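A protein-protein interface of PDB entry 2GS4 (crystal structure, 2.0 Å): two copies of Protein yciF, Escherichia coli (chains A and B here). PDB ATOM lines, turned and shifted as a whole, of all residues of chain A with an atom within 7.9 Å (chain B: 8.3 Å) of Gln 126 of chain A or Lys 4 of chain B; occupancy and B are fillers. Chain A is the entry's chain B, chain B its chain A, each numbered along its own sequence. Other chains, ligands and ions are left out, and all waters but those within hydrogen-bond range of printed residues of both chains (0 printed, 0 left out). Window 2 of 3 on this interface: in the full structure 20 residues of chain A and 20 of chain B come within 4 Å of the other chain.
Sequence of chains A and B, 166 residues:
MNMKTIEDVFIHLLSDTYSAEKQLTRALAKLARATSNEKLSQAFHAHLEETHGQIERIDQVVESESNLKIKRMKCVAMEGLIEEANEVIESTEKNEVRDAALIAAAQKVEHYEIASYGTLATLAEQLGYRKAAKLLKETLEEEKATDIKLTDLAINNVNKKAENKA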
ATOM      1  N   ILE A   6     -18.231   4.633 -29.875  1.00  0.00           N
ATOM      2  CA  ILE A   6     -19.440   5.107 -29.216  1.00  0.00           C
ATOM      3  C   ILE A   6     -19.983   6.283 -30.027  1.00  0.00           C
ATOM      4  O   ILE A   6     -21.195   6.442 -30.145  1.00  0.00           O
ATOM      5  CB  ILE A   6     -19.169   5.574 -27.751  1.00  0.00           C
ATOM      6  CG1 ILE A   6     -19.095   4.367 -26.812  1.00  0.00           C
ATOM      7  CG2 ILE A   6     -20.274   6.509 -27.273  1.00  0.00           C
ATOM      8  CD1 ILE A   6     -17.713   4.080 -26.275  1.00  0.00           C
ATOM      9  N   GLY A 118     -33.939   8.945 -24.271  1.00  0.00           N
ATOM     10  CA  GLY A 118     -33.272   8.664 -23.015  1.00  0.00           C
ATOM     11  C   GLY A 118     -31.903   8.102 -23.355  1.00  0.00           C
ATOM     12  O   GLY A 118     -30.898   8.472 -22.761  1.00  0.00           O
ATOM     13  N   THR A 119     -31.869   7.204 -24.334  1.00  0.00           N
ATOM     14  CA  THR A 119     -30.627   6.575 -24.774  1.00  0.00           C
ATOM     15  C   THR A 119     -29.665   7.573 -25.422  1.00  0.00           C
ATOM     16  O   THR A 119     -28.464   7.526 -25.172  1.00  0.00           O
ATOM     17  CB  THR A 119     -30.908   5.417 -25.764  1.00  0.00           C
ATOM     18  OG1 THR A 119     -31.639   4.380 -25.092  1.00  0.00           O
ATOM     19  CG2 THR A 119     -29.598   4.834 -26.284  1.00  0.00           C
ATOM     20  N   LEU A 120     -30.197   8.466 -26.255  1.00  0.00           N
ATOM     21  CA  LEU A 120     -29.370   9.478 -26.920  1.00  0.00           C
ATOM     22  C   LEU A 120     -28.766  10.447 -25.891  1.00  0.00           C
ATOM     23  O   LEU A 120     -27.602  10.856 -26.015  1.00  0.00           O
ATOM     24  CB  LEU A 120     -30.201  10.254 -27.969  1.00  0.00           C
ATOM     25  CG  LEU A 120     -30.512   9.589 -29.324  1.00  0.00           C
ATOM     26  CD1 LEU A 120     -31.508  10.431 -30.146  1.00  0.00           C
ATOM     27  CD2 LEU A 120     -29.221   9.416 -30.104  1.00  0.00           C
ATOM     28  N   ALA A 121     -29.553  10.787 -24.869  1.00  0.00           N
ATOM     29  CA  ALA A 121     -29.126  11.700 -23.804  1.00  0.00           C
ATOM     30  C   ALA A 121     -27.982  11.101 -22.991  1.00  0.00           C
ATOM     31  O   ALA A 121     -26.987  11.769 -22.695  1.00  0.00           O
ATOM     32  CB  ALA A 121     -30.295  12.010 -22.887  1.00  0.00           C
ATOM     33  N   THR A 122     -28.136   9.839 -22.617  1.00  0.00           N
ATOM     34  CA  THR A 122     -27.122   9.147 -21.848  1.00  0.00           C
ATOM     35  C   THR A 122     -25.838   9.029 -22.663  1.00  0.00           C
ATOM     36  O   THR A 122     -24.747   9.247 -22.141  1.00  0.00           O
ATOM     37  CB  THR A 122     -27.606   7.750 -21.443  1.00  0.00           C
ATOM     38  OG1 THR A 122     -28.747   7.875 -20.582  1.00  0.00           O
ATOM     39  CG2 THR A 122     -26.506   7.008 -20.696  1.00  0.00           C
ATOM     40  N   LEU A 123     -25.966   8.679 -23.939  1.00  0.00           N
ATOM     41  CA  LEU A 123     -24.791   8.558 -24.793  1.00  0.00           C
ATOM     42  C   LEU A 123     -24.089   9.906 -24.905  1.00  0.00           C
ATOM     43  O   LEU A 123     -22.859   9.986 -24.801  1.00  0.00           O
ATOM     44  CB  LEU A 123     -25.177   8.048 -26.187  1.00  0.00           C
ATOM     45  CG  LEU A 123     -25.502   6.559 -26.332  1.00  0.00           C
ATOM     46  CD1 LEU A 123     -26.040   6.302 -27.727  1.00  0.00           C
ATOM     47  CD2 LEU A 123     -24.245   5.720 -26.078  1.00  0.00           C
ATOM     48  N   ALA A 124     -24.875  10.957 -25.127  1.00  0.00           N
ATOM     49  CA  ALA A 124     -24.327  12.301 -25.247  1.00  0.00           C
ATOM     50  C   ALA A 124     -23.530  12.671 -24.001  1.00  0.00           C
ATOM     51  O   ALA A 124     -22.437  13.245 -24.100  1.00  0.00           O
ATOM     52  CB  ALA A 124     -25.443  13.308 -25.474  1.00  0.00           C
ATOM     53  N   GLU A 125     -24.056  12.332 -22.826  1.00  0.00           N
ATOM     54  CA  GLU A 125     -23.345  12.657 -21.597  1.00  0.00           C
ATOM     55  C   GLU A 125     -22.109  11.788 -21.411  1.00  0.00           C
ATOM     56  O   GLU A 125     -21.095  12.241 -20.889  1.00  0.00           O
ATOM     57  CB  GLU A 125     -24.269  12.552 -20.379  1.00  0.00           C
ATOM     58  CG  GLU A 125     -25.017  11.243 -20.212  1.00  0.00           C
ATOM     59  CD  GLU A 125     -26.131  11.368 -19.183  1.00  0.00           C
ATOM     60  OE1 GLU A 125     -26.775  10.345 -18.861  1.00  0.00           O
ATOM     61  OE2 GLU A 125     -26.362  12.499 -18.700  1.00  0.00           O
ATOM     62  N   GLN A 126     -22.180  10.539 -21.849  1.00  0.00           N
ATOM     63  CA  GLN A 126     -21.031   9.661 -21.715  1.00  0.00           C
ATOM     64  C   GLN A 126     -19.935  10.060 -22.712  1.00  0.00           C
ATOM     65  O   GLN A 126     -18.762   9.760 -22.510  1.00  0.00           O
ATOM     66  CB  GLN A 126     -21.473   8.202 -21.887  1.00  0.00           C
ATOM     67  CG  GLN A 126     -22.242   7.659 -20.667  1.00  0.00           C
ATOM     68  CD  GLN A 126     -21.395   7.632 -19.408  1.00  0.00           C
ATOM     69  OE1 GLN A 126     -20.202   7.330 -19.461  1.00  0.00           O
ATOM     70  NE2 GLN A 126     -22.009   7.937 -18.266  1.00  0.00           N
ATOM     71  N   LEU A 127     -20.323  10.761 -23.771  1.00  0.00           N
ATOM     72  CA  LEU A 127     -19.382  11.232 -24.788  1.00  0.00           C
ATOM     73  C   LEU A 127     -18.771  12.577 -24.397  1.00  0.00           C
ATOM     74  O   LEU A 127     -17.776  13.015 -24.988  1.00  0.00           O
ATOM     75  CB  LEU A 127     -20.085  11.377 -26.141  1.00  0.00           C
ATOM     76  CG  LEU A 127     -20.293  10.081 -26.918  1.00  0.00           C
ATOM     77  CD1 LEU A 127     -21.424  10.234 -27.913  1.00  0.00           C
ATOM     78  CD2 LEU A 127     -18.990   9.710 -27.612  1.00  0.00           C
ATOM     79  N   GLY A 128     -19.365  13.227 -23.401  1.00  0.00           N
ATOM     80  CA  GLY A 128     -18.856  14.516 -22.969  1.00  0.00           C
ATOM     81  C   GLY A 128     -19.464  15.646 -23.784  1.00  0.00           C
ATOM     82  O   GLY A 128     -18.992  16.779 -23.734  1.00  0.00           O
ATOM     83  N   TYR A 129     -20.506  15.322 -24.548  1.00  0.00           N
ATOM     84  CA  TYR A 129     -21.214  16.294 -25.385  1.00  0.00           C
ATOM     85  C   TYR A 129     -22.193  17.074 -24.511  1.00  0.00           C
ATOM     86  O   TYR A 129     -23.396  16.797 -24.527  1.00  0.00           O
ATOM     87  CB  TYR A 129     -22.017  15.582 -26.482  1.00  0.00           C
ATOM     88  CG  TYR A 129     -21.189  14.902 -27.545  1.00  0.00           C
ATOM     89  CD1 TYR A 129     -19.824  15.162 -27.668  1.00  0.00           C
ATOM     90  CD2 TYR A 129     -21.777  14.022 -28.456  1.00  0.00           C
ATOM     91  CE1 TYR A 129     -19.067  14.565 -28.672  1.00  0.00           C
ATOM     92  CE2 TYR A 129     -21.026  13.422 -29.464  1.00  0.00           C
ATOM     93  CZ  TYR A 129     -19.673  13.698 -29.564  1.00  0.00           C
ATOM     94  OH  TYR A 129     -18.920  13.110 -30.553  1.00  0.00           O
ATOM     95  N   ARG A 130     -21.698  18.066 -23.777  1.00  0.00           N
ATOM     96  CA  ARG A 130     -22.565  18.815 -22.879  1.00  0.00           C
ATOM     97  C   ARG A 130     -23.776  19.540 -23.468  1.00  0.00           C
ATOM     98  O   ARG A 130     -24.871  19.432 -22.916  1.00  0.00           O
ATOM     99  CB  ARG A 130     -21.761  19.809 -22.035  1.00  0.00           C
ATOM    100  CG  ARG A 130     -22.509  20.134 -20.749  1.00  0.00           C
ATOM    101  CD  ARG A 130     -21.991  21.354 -20.012  1.00  0.00           C
ATOM    102  NE  ARG A 130     -20.590  21.241 -19.625  1.00  0.00           N
ATOM    103  CZ  ARG A 130     -19.608  21.916 -20.209  1.00  0.00           C
ATOM    104  NH1 ARG A 130     -19.881  22.749 -21.206  1.00  0.00           N
ATOM    105  NH2 ARG A 130     -18.359  21.769 -19.792  1.00  0.00           N
ATOM    106  N   ALA A 133     -26.310  16.912 -24.703  1.00  0.00           N
ATOM    107  CA  ALA A 133     -27.014  16.255 -23.612  1.00  0.00           C
ATOM    108  C   ALA A 133     -28.197  17.132 -23.219  1.00  0.00           C
ATOM    109  O   ALA A 133     -29.331  16.657 -23.148  1.00  0.00           O
ATOM    110  CB  ALA A 133     -26.082  16.055 -22.422  1.00  0.00           C
ATOM    111  N   MET B   3     -29.818   3.599 -16.649  1.00  0.00           N
ATOM    112  CA  MET B   3     -29.922   4.808 -17.514  1.00  0.00           C
ATOM    113  C   MET B   3     -28.903   5.924 -17.257  1.00  0.00           C
ATOM    114  O   MET B   3     -29.283   7.093 -17.203  1.00  0.00           O
ATOM    115  CB  MET B   3     -31.339   5.408 -17.433  1.00  0.00           C
ATOM    116  CG  MET B   3     -31.997   5.443 -16.041  1.00  0.00           C
ATOM    117  SD  MET B   3     -30.906   5.816 -14.471  1.00  0.00           S
ATOM    118  CE  MET B   3     -30.552   7.703 -14.685  1.00  0.00           C
ATOM    119  N   LYS B   4     -27.622   5.587 -17.106  1.00  0.00           N
ATOM    120  CA  LYS B   4     -26.594   6.615 -16.889  1.00  0.00           C
ATOM    121  C   LYS B   4     -25.229   6.207 -17.434  1.00  0.00           C
ATOM    122  O   LYS B   4     -24.416   7.057 -17.790  1.00  0.00           O
ATOM    123  CB  LYS B   4     -26.476   6.986 -15.395  1.00  0.00           C
ATOM    124  CG  LYS B   4     -25.332   7.983 -15.043  1.00  0.00           C
ATOM    125  CD  LYS B   4     -25.461   8.533 -13.605  1.00  0.00           C
ATOM    126  CE  LYS B   4     -24.230   9.336 -13.140  1.00  0.00           C
ATOM    127  NZ  LYS B   4     -23.112   8.496 -12.594  1.00  0.00           N
ATOM    128  N   THR B   5     -24.976   4.907 -17.511  1.00  0.00           N
ATOM    129  CA  THR B   5     -23.698   4.433 -18.029  1.00  0.00           C
ATOM    130  C   THR B   5     -23.924   3.708 -19.349  1.00  0.00           C
ATOM    131  O   THR B   5     -25.060   3.367 -19.691  1.00  0.00           O
ATOM    132  CB  THR B   5     -23.009   3.461 -17.051  1.00  0.00           C
ATOM    133  OG1 THR B   5     -23.723   2.220 -17.026  1.00  0.00           O
ATOM    134  CG2 THR B   5     -22.992   4.049 -15.647  1.00  0.00           C
ATOM    135  N   ILE B   6     -22.841   3.491 -20.086  1.00  0.00           N
ATOM    136  CA  ILE B   6     -22.887   2.800 -21.370  1.00  0.00           C
ATOM    137  C   ILE B   6     -23.452   1.416 -21.106  1.00  0.00           C
ATOM    138  O   ILE B   6     -24.196   0.843 -21.900  1.00  0.00           O
ATOM    139  CB  ILE B   6     -21.462   2.677 -21.943  1.00  0.00           C
ATOM    140  CG1 ILE B   6     -20.897   4.077 -22.198  1.00  0.00           C
ATOM    141  CG2 ILE B   6     -21.458   1.823 -23.204  1.00  0.00           C
ATOM    142  CD1 ILE B   6     -21.823   4.983 -22.996  1.00  0.00           C
ATOM    143  N   GLU B   7     -23.082   0.915 -19.939  1.00  0.00           N
ATOM    144  CA  GLU B   7     -23.492  -0.383 -19.457  1.00  0.00           C
ATOM    145  C   GLU B   7     -25.019  -0.454 -19.329  1.00  0.00           C
ATOM    146  O   GLU B   7     -25.631  -1.431 -19.765  1.00  0.00           O
ATOM    147  CB  GLU B   7     -22.809  -0.629 -18.111  1.00  0.00           C
ATOM    148  CG  GLU B   7     -22.150  -1.975 -18.007  1.00  0.00           C
ATOM    149  CD  GLU B   7     -23.129  -3.073 -18.303  1.00  0.00           C
ATOM    150  OE1 GLU B   7     -24.277  -2.960 -17.829  1.00  0.00           O
ATOM    151  OE2 GLU B   7     -22.760  -4.040 -18.999  1.00  0.00           O
ATOM    152  N   ASP B   8     -25.636   0.571 -18.739  1.00  0.00           N
ATOM    153  CA  ASP B   8     -27.095   0.583 -18.599  1.00  0.00           C
ATOM    154  C   ASP B   8     -27.740   0.602 -19.983  1.00  0.00           C
ATOM    155  O   ASP B   8     -28.732  -0.081 -20.221  1.00  0.00           O
ATOM    156  CB  ASP B   8     -27.606   1.814 -17.839  1.00  0.00           C
ATOM    157  CG  ASP B   8     -27.144   1.871 -16.392  1.00  0.00           C
ATOM    158  OD1 ASP B   8     -27.086   0.821 -15.716  1.00  0.00           O
ATOM    159  OD2 ASP B   8     -26.862   2.995 -15.924  1.00  0.00           O
ATOM    160  N   VAL B   9     -27.180   1.401 -20.893  1.00  0.00           N
ATOM    161  CA  VAL B   9     -27.709   1.491 -22.254  1.00  0.00           C
ATOM    162  C   VAL B   9     -27.598   0.123 -22.914  1.00  0.00           C
ATOM    163  O   VAL B   9     -28.533  -0.336 -23.565  1.00  0.00           O
ATOM    164  CB  VAL B   9     -26.928   2.516 -23.127  1.00  0.00           C
ATOM    165  CG1 VAL B   9     -27.427   2.455 -24.576  1.00  0.00           C
ATOM    166  CG2 VAL B   9     -27.115   3.927 -22.590  1.00  0.00           C
ATOM    167  N   LEU B 127     -17.289  -1.748 -24.399  1.00  0.00           N
ATOM    168  CA  LEU B 127     -17.356  -1.945 -22.952  1.00  0.00           C
ATOM    169  C   LEU B 127     -16.334  -2.989 -22.503  1.00  0.00           C
ATOM    170  O   LEU B 127     -16.230  -3.303 -21.322  1.00  0.00           O
ATOM    171  CB  LEU B 127     -18.766  -2.371 -22.532  1.00  0.00           C
ATOM    172  CG  LEU B 127     -19.856  -1.291 -22.556  1.00  0.00           C
ATOM    173  CD1 LEU B 127     -21.228  -1.938 -22.647  1.00  0.00           C
ATOM    174  CD2 LEU B 127     -19.750  -0.428 -21.307  1.00  0.00           C
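Of the printed residues of chain B, Thr 122 of chain A touches Met 3, Lys 4 and Val 9. Of the printed residues of chain B, Leu 123 of chain A touches Ile 6 (3.99 Å). Of the printed residues of chain A, Met 3 of chain B touches Thr 122 (3.5 Å). Lys 4 of chain B touches just these residues of chain A: Thr 122 (3.6 Å) and Gln 126 (2.6 Å). Of the printed residues of chain A, Thr 5 of chain B touches Gln 126. Printed residues of chain A within 4 Å of Val 9 of chain B: Thr 119 (3.6 Å) and Thr 122 (3.7 Å). The nearest residue of chain B that does not touch Gln 126 of chain A is Val 9 of chain B (6.4 Å).
The backbone NH (N) of Lys 4 of chain B is in hydrogen-bond range of the side-chain carboxylate (OD2) of Asp 8 of chain B (2.9 Å). The backbone carbonyl oxygen (O) of Gly 118 of chain A lies within hydrogen-bond range of the side-chain hydroxyl (OG1) of Thr 122 of chain A (3.1 Å). The backbone NH (N) of Met 3 of chain B sits close to the side-chain carboxylate (OD2) of Asp 8 of chain B (3.1 Å). The side-chain hydroxyl (OG1) of Thr 5 of chain B sits close to the backbone NH (N) of Glu 7 of chain B. The backbone NH of Asp 8 of chain B lies within hydrogen-bond range of the side-chain hydroxyl of Thr 5 of chain B (3.1 Å).
NE2 of Gln 126 of chain A is in hydrogen-bond range of O of Lys 4 of chain B (2.6 Å).
Printed residues of chain B that touch a printed residue of chain A: Met 3, Lys 4, Thr 5, Ile 6 and Val 9. Hydrophobic or aromatic side chains of chain B that line the printed part of chain A: Ile 6 and Val 9. Along chain B the printed residues that touch a printed residue of chain A span positions 3 to 9. Among the printed residues, 8 pairs touch across the chains.
Val 9 of chain B touches Thr 119 of chain A (CG1 to CG2, 3.6 Å). O of Met 3 of chain B touches OG1 of Thr 122 of chain A, at 3.5 Å. O of Lys 4 of chain B touches CG2 of Thr 122 of chain A (3.6 Å). Val 9 of chain B touches Thr 122 of chain A (CG2 to CG2, 3.7 Å). Leu 123 of chain A touches Ile 6 of chain B. Thr 5 of chain B touches Gln 126 of chain A. CD1 of Ile 6 of chain B touches CB of Gln 126 of chain A (3.4 Å).
Positions printed for both chains: 6 and 127. Of the 8 pairs that touch across the chains among the printed residues, none has its exchanged pair printed and touching as well.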
